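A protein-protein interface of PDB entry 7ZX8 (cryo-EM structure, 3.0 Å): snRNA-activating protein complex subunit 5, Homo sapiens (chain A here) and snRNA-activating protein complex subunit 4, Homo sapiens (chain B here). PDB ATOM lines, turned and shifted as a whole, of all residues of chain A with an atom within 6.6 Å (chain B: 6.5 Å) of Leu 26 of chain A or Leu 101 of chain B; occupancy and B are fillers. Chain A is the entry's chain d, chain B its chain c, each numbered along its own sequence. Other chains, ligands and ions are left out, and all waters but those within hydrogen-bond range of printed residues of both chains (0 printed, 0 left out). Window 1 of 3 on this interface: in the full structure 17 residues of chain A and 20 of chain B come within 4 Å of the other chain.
The backbone carbonyl oxygen of Ala 104 of chain B sits at hydrogen-bond distance from the side-chain amino group of Lys 19 of chain A.
OD1 of Asn 105 of chain B sits close to O of Leu 101 of chain B, 2.7 Å away.
A ring nitrogen (ND1) of His 23 of chain A lies within hydrogen-bond range of the backbone carbonyl oxygen (O) of Lys 19 of chain A.
The backbone carbonyl oxygen (O) of His 23 of chain A lies close to the side-chain amide oxygen (OD1) of Asn 27 of chain A, 3.0 Å away.
The side-chain amide oxygen of Gln 25 of chain A lies within hydrogen-bond range of the guanidinium group of Arg 28 of chain A (3.1 Å).
Among the printed residues, pairs that only touch across the chains: Lys 19 of chain A with Asn 105 of chain B (3.2 Å), Leu 22 of chain A with Ile 97 of chain B (3.4 Å), Leu 22 of chain A with Lys 100 of chain B (3.9 Å), Leu 22 of chain A with Leu 101 of chain B (3.3 Å), His 23 of chain A with Leu 101 of chain B (3.8 Å), Gln 25 of chain A with Tyr 93 of chain B (3.99 Å), Gln 25 of chain A with Ile 97 of chain B (3.5 Å), Leu 26 of chain A with Ile 97 of chain B (3.4 Å), Leu 26 of chain A with Leu 101 of chain B (3.2 Å), Leu 29 of chain A with Tyr 93 of chain B (3.5 Å), Leu 29 of chain A with Gln 94 of chain B (3.6 Å) and Lys 30 of chain A with Gln 94 of chain B (3.5 Å).
Of the printed residues of chain B, Leu 26 of chain A touches Ile 97 (3.4 Å) and Leu 101 (3.2 Å).
Leu 101 of chain B touches three residues of chain A.
Of the printed residues of chain A, Asn 105 of chain B touches Lys 19.
Of the printed residues of chain B, Leu 22 of chain A touches Ile 97, Lys 100 and Leu 101.
Printed residues of chain A within 4 Å of Gln 94 of chain B: Leu 29 (3.6 Å) and Lys 30 (3.5 Å).
Ala 21 of chain A touches none of the printed residues of chain B.
Glu 103 of chain B touches none of the printed residues of chain A.
The nearest printed residue of chain B that does not touch Leu 26 of chain A is Gln 98 of chain B (4.1 Å).
The nearest residue of chain A that does not touch Leu 101 of chain B is Lys 19 of chain A (4.7 Å).
The nearest printed residue of chain A that does not touch Tyr 93 of chain B is Leu 26 of chain A (6.0 Å).
Of the 13 printed residues of chain A, 7 touch a printed residue of chain B.
Printed residues of chain A that touch a printed residue of chain B: Lys 19, Leu 22, His 23, Gln 25, Leu 26, Leu 29 and Lys 30.
Hydrophobic or aromatic side chains of chain A within 4 Å of the printed part of chain B: Leu 22, His 23, Leu 26 and Leu 29.
Of the 13 printed residues of chain B, 7 touch a printed residue of chain A.
Printed residues of chain B that touch a printed residue of chain A: Tyr 93, Gln 94, Ile 97, Lys 100, Leu 101, Ala 104 and Asn 105.
Among the printed residues, 13 pairs touch across the chains.
Among the printed residues, no Asp or Glu carboxylate lies within 4 Å of a Lys or Arg side-chain nitrogen of the other chain.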
ATOM      1  N   LEU A  18     -22.878  -4.394 -26.372  1.00  0.00           N
ATOM      2  CA  LEU A  18     -22.123  -5.484 -25.761  1.00  0.00           C
ATOM      3  C   LEU A  18     -22.116  -5.358 -24.242  1.00  0.00           C
ATOM      4  O   LEU A  18     -22.299  -6.352 -23.528  1.00  0.00           O
ATOM      5  CB  LEU A  18     -20.696  -5.506 -26.310  1.00  0.00           C
ATOM      6  CG  LEU A  18     -20.556  -5.737 -27.818  1.00  0.00           C
ATOM      7  CD1 LEU A  18     -19.098  -5.638 -28.244  1.00  0.00           C
ATOM      8  CD2 LEU A  18     -21.137  -7.086 -28.220  1.00  0.00           C
ATOM      9  N   LYS A  19     -21.920  -4.140 -23.728  1.00  0.00           N
ATOM     10  CA  LYS A  19     -21.938  -3.932 -22.285  1.00  0.00           C
ATOM     11  C   LYS A  19     -23.310  -4.226 -21.695  1.00  0.00           C
ATOM     12  O   LYS A  19     -23.408  -4.788 -20.604  1.00  0.00           O
ATOM     13  CB  LYS A  19     -21.512  -2.503 -21.951  1.00  0.00           C
ATOM     14  CG  LYS A  19     -20.049  -2.205 -22.208  1.00  0.00           C
ATOM     15  CD  LYS A  19     -19.729  -0.765 -21.850  1.00  0.00           C
ATOM     16  CE  LYS A  19     -18.249  -0.475 -21.975  1.00  0.00           C
ATOM     17  NZ  LYS A  19     -17.788  -0.557 -23.386  1.00  0.00           N
ATOM     18  N   ALA A  21     -25.587  -6.371 -22.849  1.00  0.00           N
ATOM     19  CA  ALA A  21     -25.752  -7.820 -22.819  1.00  0.00           C
ATOM     20  C   ALA A  21     -24.927  -8.438 -21.699  1.00  0.00           C
ATOM     21  O   ALA A  21     -25.421  -9.287 -20.944  1.00  0.00           O
ATOM     22  CB  ALA A  21     -25.361  -8.423 -24.167  1.00  0.00           C
ATOM     23  N   LEU A  22     -23.672  -8.008 -21.553  1.00  0.00           N
ATOM     24  CA  LEU A  22     -22.820  -8.634 -20.551  1.00  0.00           C
ATOM     25  C   LEU A  22     -23.254  -8.229 -19.147  1.00  0.00           C
ATOM     26  O   LEU A  22     -23.040  -8.977 -18.192  1.00  0.00           O
ATOM     27  CB  LEU A  22     -21.361  -8.250 -20.776  1.00  0.00           C
ATOM     28  CG  LEU A  22     -20.372  -9.028 -19.900  1.00  0.00           C
ATOM     29  CD1 LEU A  22     -19.014  -9.082 -20.596  1.00  0.00           C
ATOM     30  CD2 LEU A  22     -20.273  -8.561 -18.453  1.00  0.00           C
ATOM     31  N   HIS A  23     -23.854  -7.046 -18.997  1.00  0.00           N
ATOM     32  CA  HIS A  23     -24.357  -6.634 -17.694  1.00  0.00           C
ATOM     33  C   HIS A  23     -25.585  -7.441 -17.310  1.00  0.00           C
ATOM     34  O   HIS A  23     -25.756  -7.804 -16.141  1.00  0.00           O
ATOM     35  CB  HIS A  23     -24.677  -5.140 -17.701  1.00  0.00           C
ATOM     36  CG  HIS A  23     -23.465  -4.260 -17.671  1.00  0.00           C
ATOM     37  ND1 HIS A  23     -23.321  -3.164 -18.494  1.00  0.00           N
ATOM     38  CD2 HIS A  23     -22.338  -4.319 -16.923  1.00  0.00           C
ATOM     39  CE1 HIS A  23     -22.160  -2.582 -18.250  1.00  0.00           C
ATOM     40  NE2 HIS A  23     -21.544  -3.264 -17.301  1.00  0.00           N
ATOM     41  N   ASP A  24     -26.453  -7.738 -18.280  1.00  0.00           N
ATOM     42  CA  ASP A  24     -27.509  -8.711 -18.024  1.00  0.00           C
ATOM     43  C   ASP A  24     -26.908 -10.048 -17.608  1.00  0.00           C
ATOM     44  O   ASP A  24     -27.404 -10.706 -16.681  1.00  0.00           O
ATOM     45  CB  ASP A  24     -28.386  -8.875 -19.266  1.00  0.00           C
ATOM     46  CG  ASP A  24     -29.586  -9.769 -19.018  1.00  0.00           C
ATOM     47  OD1 ASP A  24     -30.537  -9.319 -18.348  1.00  0.00           O
ATOM     48  OD2 ASP A  24     -29.575 -10.925 -19.492  1.00  0.00           O
ATOM     49  N   GLN A  25     -25.823 -10.452 -18.274  1.00  0.00           N
ATOM     50  CA  GLN A  25     -25.149 -11.700 -17.926  1.00  0.00           C
ATOM     51  C   GLN A  25     -24.651 -11.679 -16.485  1.00  0.00           C
ATOM     52  O   GLN A  25     -24.814 -12.654 -15.747  1.00  0.00           O
ATOM     53  CB  GLN A  25     -23.993 -11.957 -18.895  1.00  0.00           C
ATOM     54  CG  GLN A  25     -23.185 -13.216 -18.601  1.00  0.00           C
ATOM     55  CD  GLN A  25     -24.046 -14.460 -18.499  1.00  0.00           C
ATOM     56  OE1 GLN A  25     -24.779 -14.644 -17.528  1.00  0.00           O
ATOM     57  NE2 GLN A  25     -23.957 -15.325 -19.503  1.00  0.00           N
ATOM     58  N   LEU A  26     -24.032 -10.574 -16.065  1.00  0.00           N
ATOM     59  CA  LEU A  26     -23.535 -10.487 -14.693  1.00  0.00           C
ATOM     60  C   LEU A  26     -24.672 -10.433 -13.680  1.00  0.00           C
ATOM     61  O   LEU A  26     -24.561 -11.008 -12.595  1.00  0.00           O
ATOM     62  CB  LEU A  26     -22.623  -9.273 -14.516  1.00  0.00           C
ATOM     63  CG  LEU A  26     -21.154  -9.436 -14.894  1.00  0.00           C
ATOM     64  CD1 LEU A  26     -20.409  -8.155 -14.569  1.00  0.00           C
ATOM     65  CD2 LEU A  26     -20.533 -10.620 -14.159  1.00  0.00           C
ATOM     66  N   ASN A  27     -25.758  -9.726 -13.991  1.00  0.00           N
ATOM     67  CA  ASN A  27     -26.880  -9.674 -13.059  1.00  0.00           C
ATOM     68  C   ASN A  27     -27.465 -11.064 -12.843  1.00  0.00           C
ATOM     69  O   ASN A  27     -27.688 -11.491 -11.702  1.00  0.00           O
ATOM     70  CB  ASN A  27     -27.949  -8.709 -13.574  1.00  0.00           C
ATOM     71  CG  ASN A  27     -27.404  -7.317 -13.826  1.00  0.00           C
ATOM     72  OD1 ASN A  27     -26.363  -6.938 -13.288  1.00  0.00           O
ATOM     73  ND2 ASN A  27     -28.105  -6.545 -14.649  1.00  0.00           N
ATOM     74  N   ARG A  28     -27.698 -11.798 -13.932  1.00  0.00           N
ATOM     75  CA  ARG A  28     -28.197 -13.163 -13.793  1.00  0.00           C
ATOM     76  C   ARG A  28     -27.163 -14.073 -13.136  1.00  0.00           C
ATOM     77  O   ARG A  28     -27.530 -14.968 -12.366  1.00  0.00           O
ATOM     78  CB  ARG A  28     -28.624 -13.697 -15.160  1.00  0.00           C
ATOM     79  CG  ARG A  28     -27.522 -13.721 -16.195  1.00  0.00           C
ATOM     80  CD  ARG A  28     -28.088 -13.805 -17.596  1.00  0.00           C
ATOM     81  NE  ARG A  28     -28.956 -14.961 -17.758  1.00  0.00           N
ATOM     82  CZ  ARG A  28     -28.518 -16.209 -17.870  1.00  0.00           C
ATOM     83  NH1 ARG A  28     -27.218 -16.472 -17.837  1.00  0.00           N
ATOM     84  NH2 ARG A  28     -29.384 -17.195 -18.014  1.00  0.00           N
ATOM     85  N   LEU A  29     -25.875 -13.850 -13.401  1.00  0.00           N
ATOM     86  CA  LEU A  29     -24.832 -14.637 -12.753  1.00  0.00           C
ATOM     87  C   LEU A  29     -24.842 -14.420 -11.246  1.00  0.00           C
ATOM     88  O   LEU A  29     -24.704 -15.369 -10.472  1.00  0.00           O
ATOM     89  CB  LEU A  29     -23.465 -14.275 -13.336  1.00  0.00           C
ATOM     90  CG  LEU A  29     -22.999 -15.013 -14.595  1.00  0.00           C
ATOM     91  CD1 LEU A  29     -21.586 -14.580 -14.953  1.00  0.00           C
ATOM     92  CD2 LEU A  29     -23.061 -16.524 -14.419  1.00  0.00           C
ATOM     93  N   LYS A  30     -24.994 -13.169 -10.809  1.00  0.00           N
ATOM     94  CA  LYS A  30     -25.051 -12.885  -9.379  1.00  0.00           C
ATOM     95  C   LYS A  30     -26.325 -13.433  -8.753  1.00  0.00           C
ATOM     96  O   LYS A  30     -26.308 -13.861  -7.592  1.00  0.00           O
ATOM     97  CB  LYS A  30     -24.935 -11.381  -9.129  1.00  0.00           C
ATOM     98  CG  LYS A  30     -23.602 -10.785  -9.555  1.00  0.00           C
ATOM     99  CD  LYS A  30     -23.581  -9.274  -9.379  1.00  0.00           C
ATOM    100  CE  LYS A  30     -24.116  -8.554 -10.606  1.00  0.00           C
ATOM    101  NZ  LYS A  30     -23.672  -7.133 -10.654  1.00  0.00           N
ATOM    102  N   VAL A  31     -27.436 -13.429  -9.491  1.00  0.00           N
ATOM    103  CA  VAL A  31     -28.639 -14.099  -9.003  1.00  0.00           C
ATOM    104  C   VAL A  31     -28.350 -15.579  -8.773  1.00  0.00           C
ATOM    105  O   VAL A  31     -28.718 -16.156  -7.739  1.00  0.00           O
ATOM    106  CB  VAL A  31     -29.805 -13.896  -9.987  1.00  0.00           C
ATOM    107  CG1 VAL A  31     -30.975 -14.796  -9.621  1.00  0.00           C
ATOM    108  CG2 VAL A  31     -30.236 -12.437 -10.003  1.00  0.00           C
ATOM    109  N   TYR B  93     -15.310 -17.479 -13.576  1.00  0.00           N
ATOM    110  CA  TYR B  93     -16.055 -16.966 -14.722  1.00  0.00           C
ATOM    111  C   TYR B  93     -16.396 -15.492 -14.533  1.00  0.00           C
ATOM    112  O   TYR B  93     -16.258 -14.685 -15.464  1.00  0.00           O
ATOM    113  CB  TYR B  93     -17.325 -17.791 -14.930  1.00  0.00           C
ATOM    114  CG  TYR B  93     -18.082 -17.454 -16.197  1.00  0.00           C
ATOM    115  CD1 TYR B  93     -17.477 -17.571 -17.442  1.00  0.00           C
ATOM    116  CD2 TYR B  93     -19.401 -17.025 -16.148  1.00  0.00           C
ATOM    117  CE1 TYR B  93     -18.165 -17.266 -18.602  1.00  0.00           C
ATOM    118  CE2 TYR B  93     -20.097 -16.719 -17.303  1.00  0.00           C
ATOM    119  CZ  TYR B  93     -19.475 -16.841 -18.526  1.00  0.00           C
ATOM    120  OH  TYR B  93     -20.163 -16.537 -19.678  1.00  0.00           O
ATOM    121  N   GLN B  94     -16.837 -15.120 -13.329  1.00  0.00           N
ATOM    122  CA  GLN B  94     -17.119 -13.719 -13.040  1.00  0.00           C
ATOM    123  C   GLN B  94     -15.852 -12.880 -13.131  1.00  0.00           C
ATOM    124  O   GLN B  94     -15.893 -11.734 -13.582  1.00  0.00           O
ATOM    125  CB  GLN B  94     -17.754 -13.587 -11.657  1.00  0.00           C
ATOM    126  CG  GLN B  94     -19.186 -14.097 -11.582  1.00  0.00           C
ATOM    127  CD  GLN B  94     -20.022 -13.344 -10.567  1.00  0.00           C
ATOM    128  OE1 GLN B  94     -21.173 -12.995 -10.829  1.00  0.00           O
ATOM    129  NE2 GLN B  94     -19.446 -13.092  -9.396  1.00  0.00           N
ATOM    130  N   VAL B  96     -13.182 -13.417 -15.124  1.00  0.00           N
ATOM    131  CA  VAL B  96     -12.825 -13.203 -16.525  1.00  0.00           C
ATOM    132  C   VAL B  96     -13.804 -12.234 -17.183  1.00  0.00           C
ATOM    133  O   VAL B  96     -13.399 -11.330 -17.929  1.00  0.00           O
ATOM    134  CB  VAL B  96     -12.749 -14.545 -17.282  1.00  0.00           C
ATOM    135  CG1 VAL B  96     -14.064 -15.300 -17.208  1.00  0.00           C
ATOM    136  CG2 VAL B  96     -12.338 -14.321 -18.733  1.00  0.00           C
ATOM    137  N   ILE B  97     -15.101 -12.389 -16.910  1.00  0.00           N
ATOM    138  CA  ILE B  97     -16.082 -11.519 -17.549  1.00  0.00           C
ATOM    139  C   ILE B  97     -15.954 -10.091 -17.016  1.00  0.00           C
ATOM    140  O   ILE B  97     -16.191  -9.118 -17.745  1.00  0.00           O
ATOM    141  CB  ILE B  97     -17.493 -12.103 -17.343  1.00  0.00           C
ATOM    142  CG1 ILE B  97     -18.500 -11.451 -18.281  1.00  0.00           C
ATOM    143  CG2 ILE B  97     -17.950 -11.892 -15.919  1.00  0.00           C
ATOM    144  CD1 ILE B  97     -19.816 -12.200 -18.347  1.00  0.00           C
ATOM    145  N   GLN B  98     -15.550  -9.935 -15.751  1.00  0.00           N
ATOM    146  CA  GLN B  98     -15.310  -8.606 -15.198  1.00  0.00           C
ATOM    147  C   GLN B  98     -14.061  -7.971 -15.788  1.00  0.00           C
ATOM    148  O   GLN B  98     -14.023  -6.753 -15.978  1.00  0.00           O
ATOM    149  CB  GLN B  98     -15.195  -8.690 -13.676  1.00  0.00           C
ATOM    150  CG  GLN B  98     -14.834  -7.376 -12.996  1.00  0.00           C
ATOM    151  CD  GLN B  98     -15.619  -6.196 -13.534  1.00  0.00           C
ATOM    152  OE1 GLN B  98     -16.828  -6.280 -13.742  1.00  0.00           O
ATOM    153  NE2 GLN B  98     -14.929  -5.084 -13.761  1.00  0.00           N
ATOM    154  N   GLU B  99     -13.029  -8.766 -16.073  1.00  0.00           N
ATOM    155  CA  GLU B  99     -11.890  -8.238 -16.818  1.00  0.00           C
ATOM    156  C   GLU B  99     -12.329  -7.775 -18.202  1.00  0.00           C
ATOM    157  O   GLU B  99     -11.849  -6.752 -18.716  1.00  0.00           O
ATOM    158  CB  GLU B  99     -10.798  -9.304 -16.922  1.00  0.00           C
ATOM    159  CG  GLU B  99      -9.424  -8.768 -17.302  1.00  0.00           C
ATOM    160  CD  GLU B  99      -9.313  -8.419 -18.773  1.00  0.00           C
ATOM    161  OE1 GLU B  99      -9.665  -9.269 -19.618  1.00  0.00           O
ATOM    162  OE2 GLU B  99      -8.868  -7.294 -19.084  1.00  0.00           O
ATOM    163  N   LYS B 100     -13.241  -8.526 -18.824  1.00  0.00           N
ATOM    164  CA  LYS B 100     -13.779  -8.110 -20.114  1.00  0.00           C
ATOM    165  C   LYS B 100     -14.486  -6.765 -19.996  1.00  0.00           C
ATOM    166  O   LYS B 100     -14.298  -5.881 -20.839  1.00  0.00           O
ATOM    167  CB  LYS B 100     -14.730  -9.177 -20.660  1.00  0.00           C
ATOM    168  CG  LYS B 100     -15.351  -8.856 -22.020  1.00  0.00           C
ATOM    169  CD  LYS B 100     -14.304  -8.869 -23.129  1.00  0.00           C
ATOM    170  CE  LYS B 100     -14.907  -8.564 -24.494  1.00  0.00           C
ATOM    171  NZ  LYS B 100     -15.832  -9.639 -24.960  1.00  0.00           N
ATOM    172  N   LEU B 101     -15.301  -6.588 -18.952  1.00  0.00           N
ATOM    173  CA  LEU B 101     -15.920  -5.281 -18.738  1.00  0.00           C
ATOM    174  C   LEU B 101     -14.885  -4.208 -18.455  1.00  0.00           C
ATOM    175  O   LEU B 101     -15.072  -3.054 -18.833  1.00  0.00           O
ATOM    176  CB  LEU B 101     -16.932  -5.302 -17.598  1.00  0.00           C
ATOM    177  CG  LEU B 101     -18.181  -6.129 -17.809  1.00  0.00           C
ATOM    178  CD1 LEU B 101     -18.973  -6.113 -16.520  1.00  0.00           C
ATOM    179  CD2 LEU B 101     -18.960  -5.559 -18.989  1.00  0.00           C
ATOM    180  N   ALA B 102     -13.814  -4.545 -17.745  1.00  0.00           N
ATOM    181  CA  ALA B 102     -12.784  -3.549 -17.484  1.00  0.00           C
ATOM    182  C   ALA B 102     -12.219  -3.021 -18.795  1.00  0.00           C
ATOM    183  O   ALA B 102     -12.174  -1.806 -19.028  1.00  0.00           O
ATOM    184  CB  ALA B 102     -11.682  -4.160 -16.619  1.00  0.00           C
ATOM    185  N   GLU B 103     -11.832  -3.934 -19.687  1.00  0.00           N
ATOM    186  CA  GLU B 103     -11.320  -3.517 -20.989  1.00  0.00           C
ATOM    187  C   GLU B 103     -12.374  -2.738 -21.771  1.00  0.00           C
ATOM    188  O   GLU B 103     -12.079  -1.684 -22.350  1.00  0.00           O
ATOM    189  CB  GLU B 103     -10.850  -4.743 -21.775  1.00  0.00           C
ATOM    190  CG  GLU B 103      -9.976  -4.431 -22.982  1.00  0.00           C
ATOM    191  CD  GLU B 103     -10.779  -4.110 -24.227  1.00  0.00           C
ATOM    192  OE1 GLU B 103     -12.014  -4.295 -24.209  1.00  0.00           O
ATOM    193  OE2 GLU B 103     -10.172  -3.681 -25.230  1.00  0.00           O
ATOM    194  N   ALA B 104     -13.616  -3.229 -21.781  1.00  0.00           N
ATOM    195  CA  ALA B 104     -14.665  -2.589 -22.568  1.00  0.00           C
ATOM    196  C   ALA B 104     -14.999  -1.200 -22.036  1.00  0.00           C
ATOM    197  O   ALA B 104     -15.253  -0.276 -22.816  1.00  0.00           O
ATOM    198  CB  ALA B 104     -15.910  -3.473 -22.583  1.00  0.00           C
ATOM    199  N   ASN B 105     -15.014  -1.031 -20.714  1.00  0.00           N
ATOM    200  CA  ASN B 105     -15.309   0.266 -20.123  1.00  0.00           C
ATOM    201  C   ASN B 105     -14.155   1.235 -20.320  1.00  0.00           C
ATOM    202  O   ASN B 105     -14.383   2.440 -20.462  1.00  0.00           O
ATOM    203  CB  ASN B 105     -15.624   0.112 -18.634  1.00  0.00           C
ATOM    204  CG  ASN B 105     -16.948  -0.588 -18.388  1.00  0.00           C
ATOM    205  OD1 ASN B 105     -17.306  -1.531 -19.094  1.00  0.00           O
ATOM    206  ND2 ASN B 105     -17.685  -0.126 -17.384  1.00  0.00           N
ATOM    207  N   LEU B 106     -12.915   0.741 -20.333  1.00  0.00           N
ATOM    208  CA  LEU B 106     -11.807   1.603 -20.728  1.00  0.00           C
ATOM    209  C   LEU B 106     -11.965   2.063 -22.173  1.00  0.00           C
ATOM    210  O   LEU B 106     -11.716   3.232 -22.492  1.00  0.00           O
ATOM    211  CB  LEU B 106     -10.473   0.883 -20.525  1.00  0.00           C
ATOM    212  CG  LEU B 106      -9.821   0.988 -19.139  1.00  0.00           C
ATOM    213  CD1 LEU B 106      -9.445   2.435 -18.837  1.00  0.00           C
ATOM    214  CD2 LEU B 106     -10.699   0.427 -18.023  1.00  0.00           C
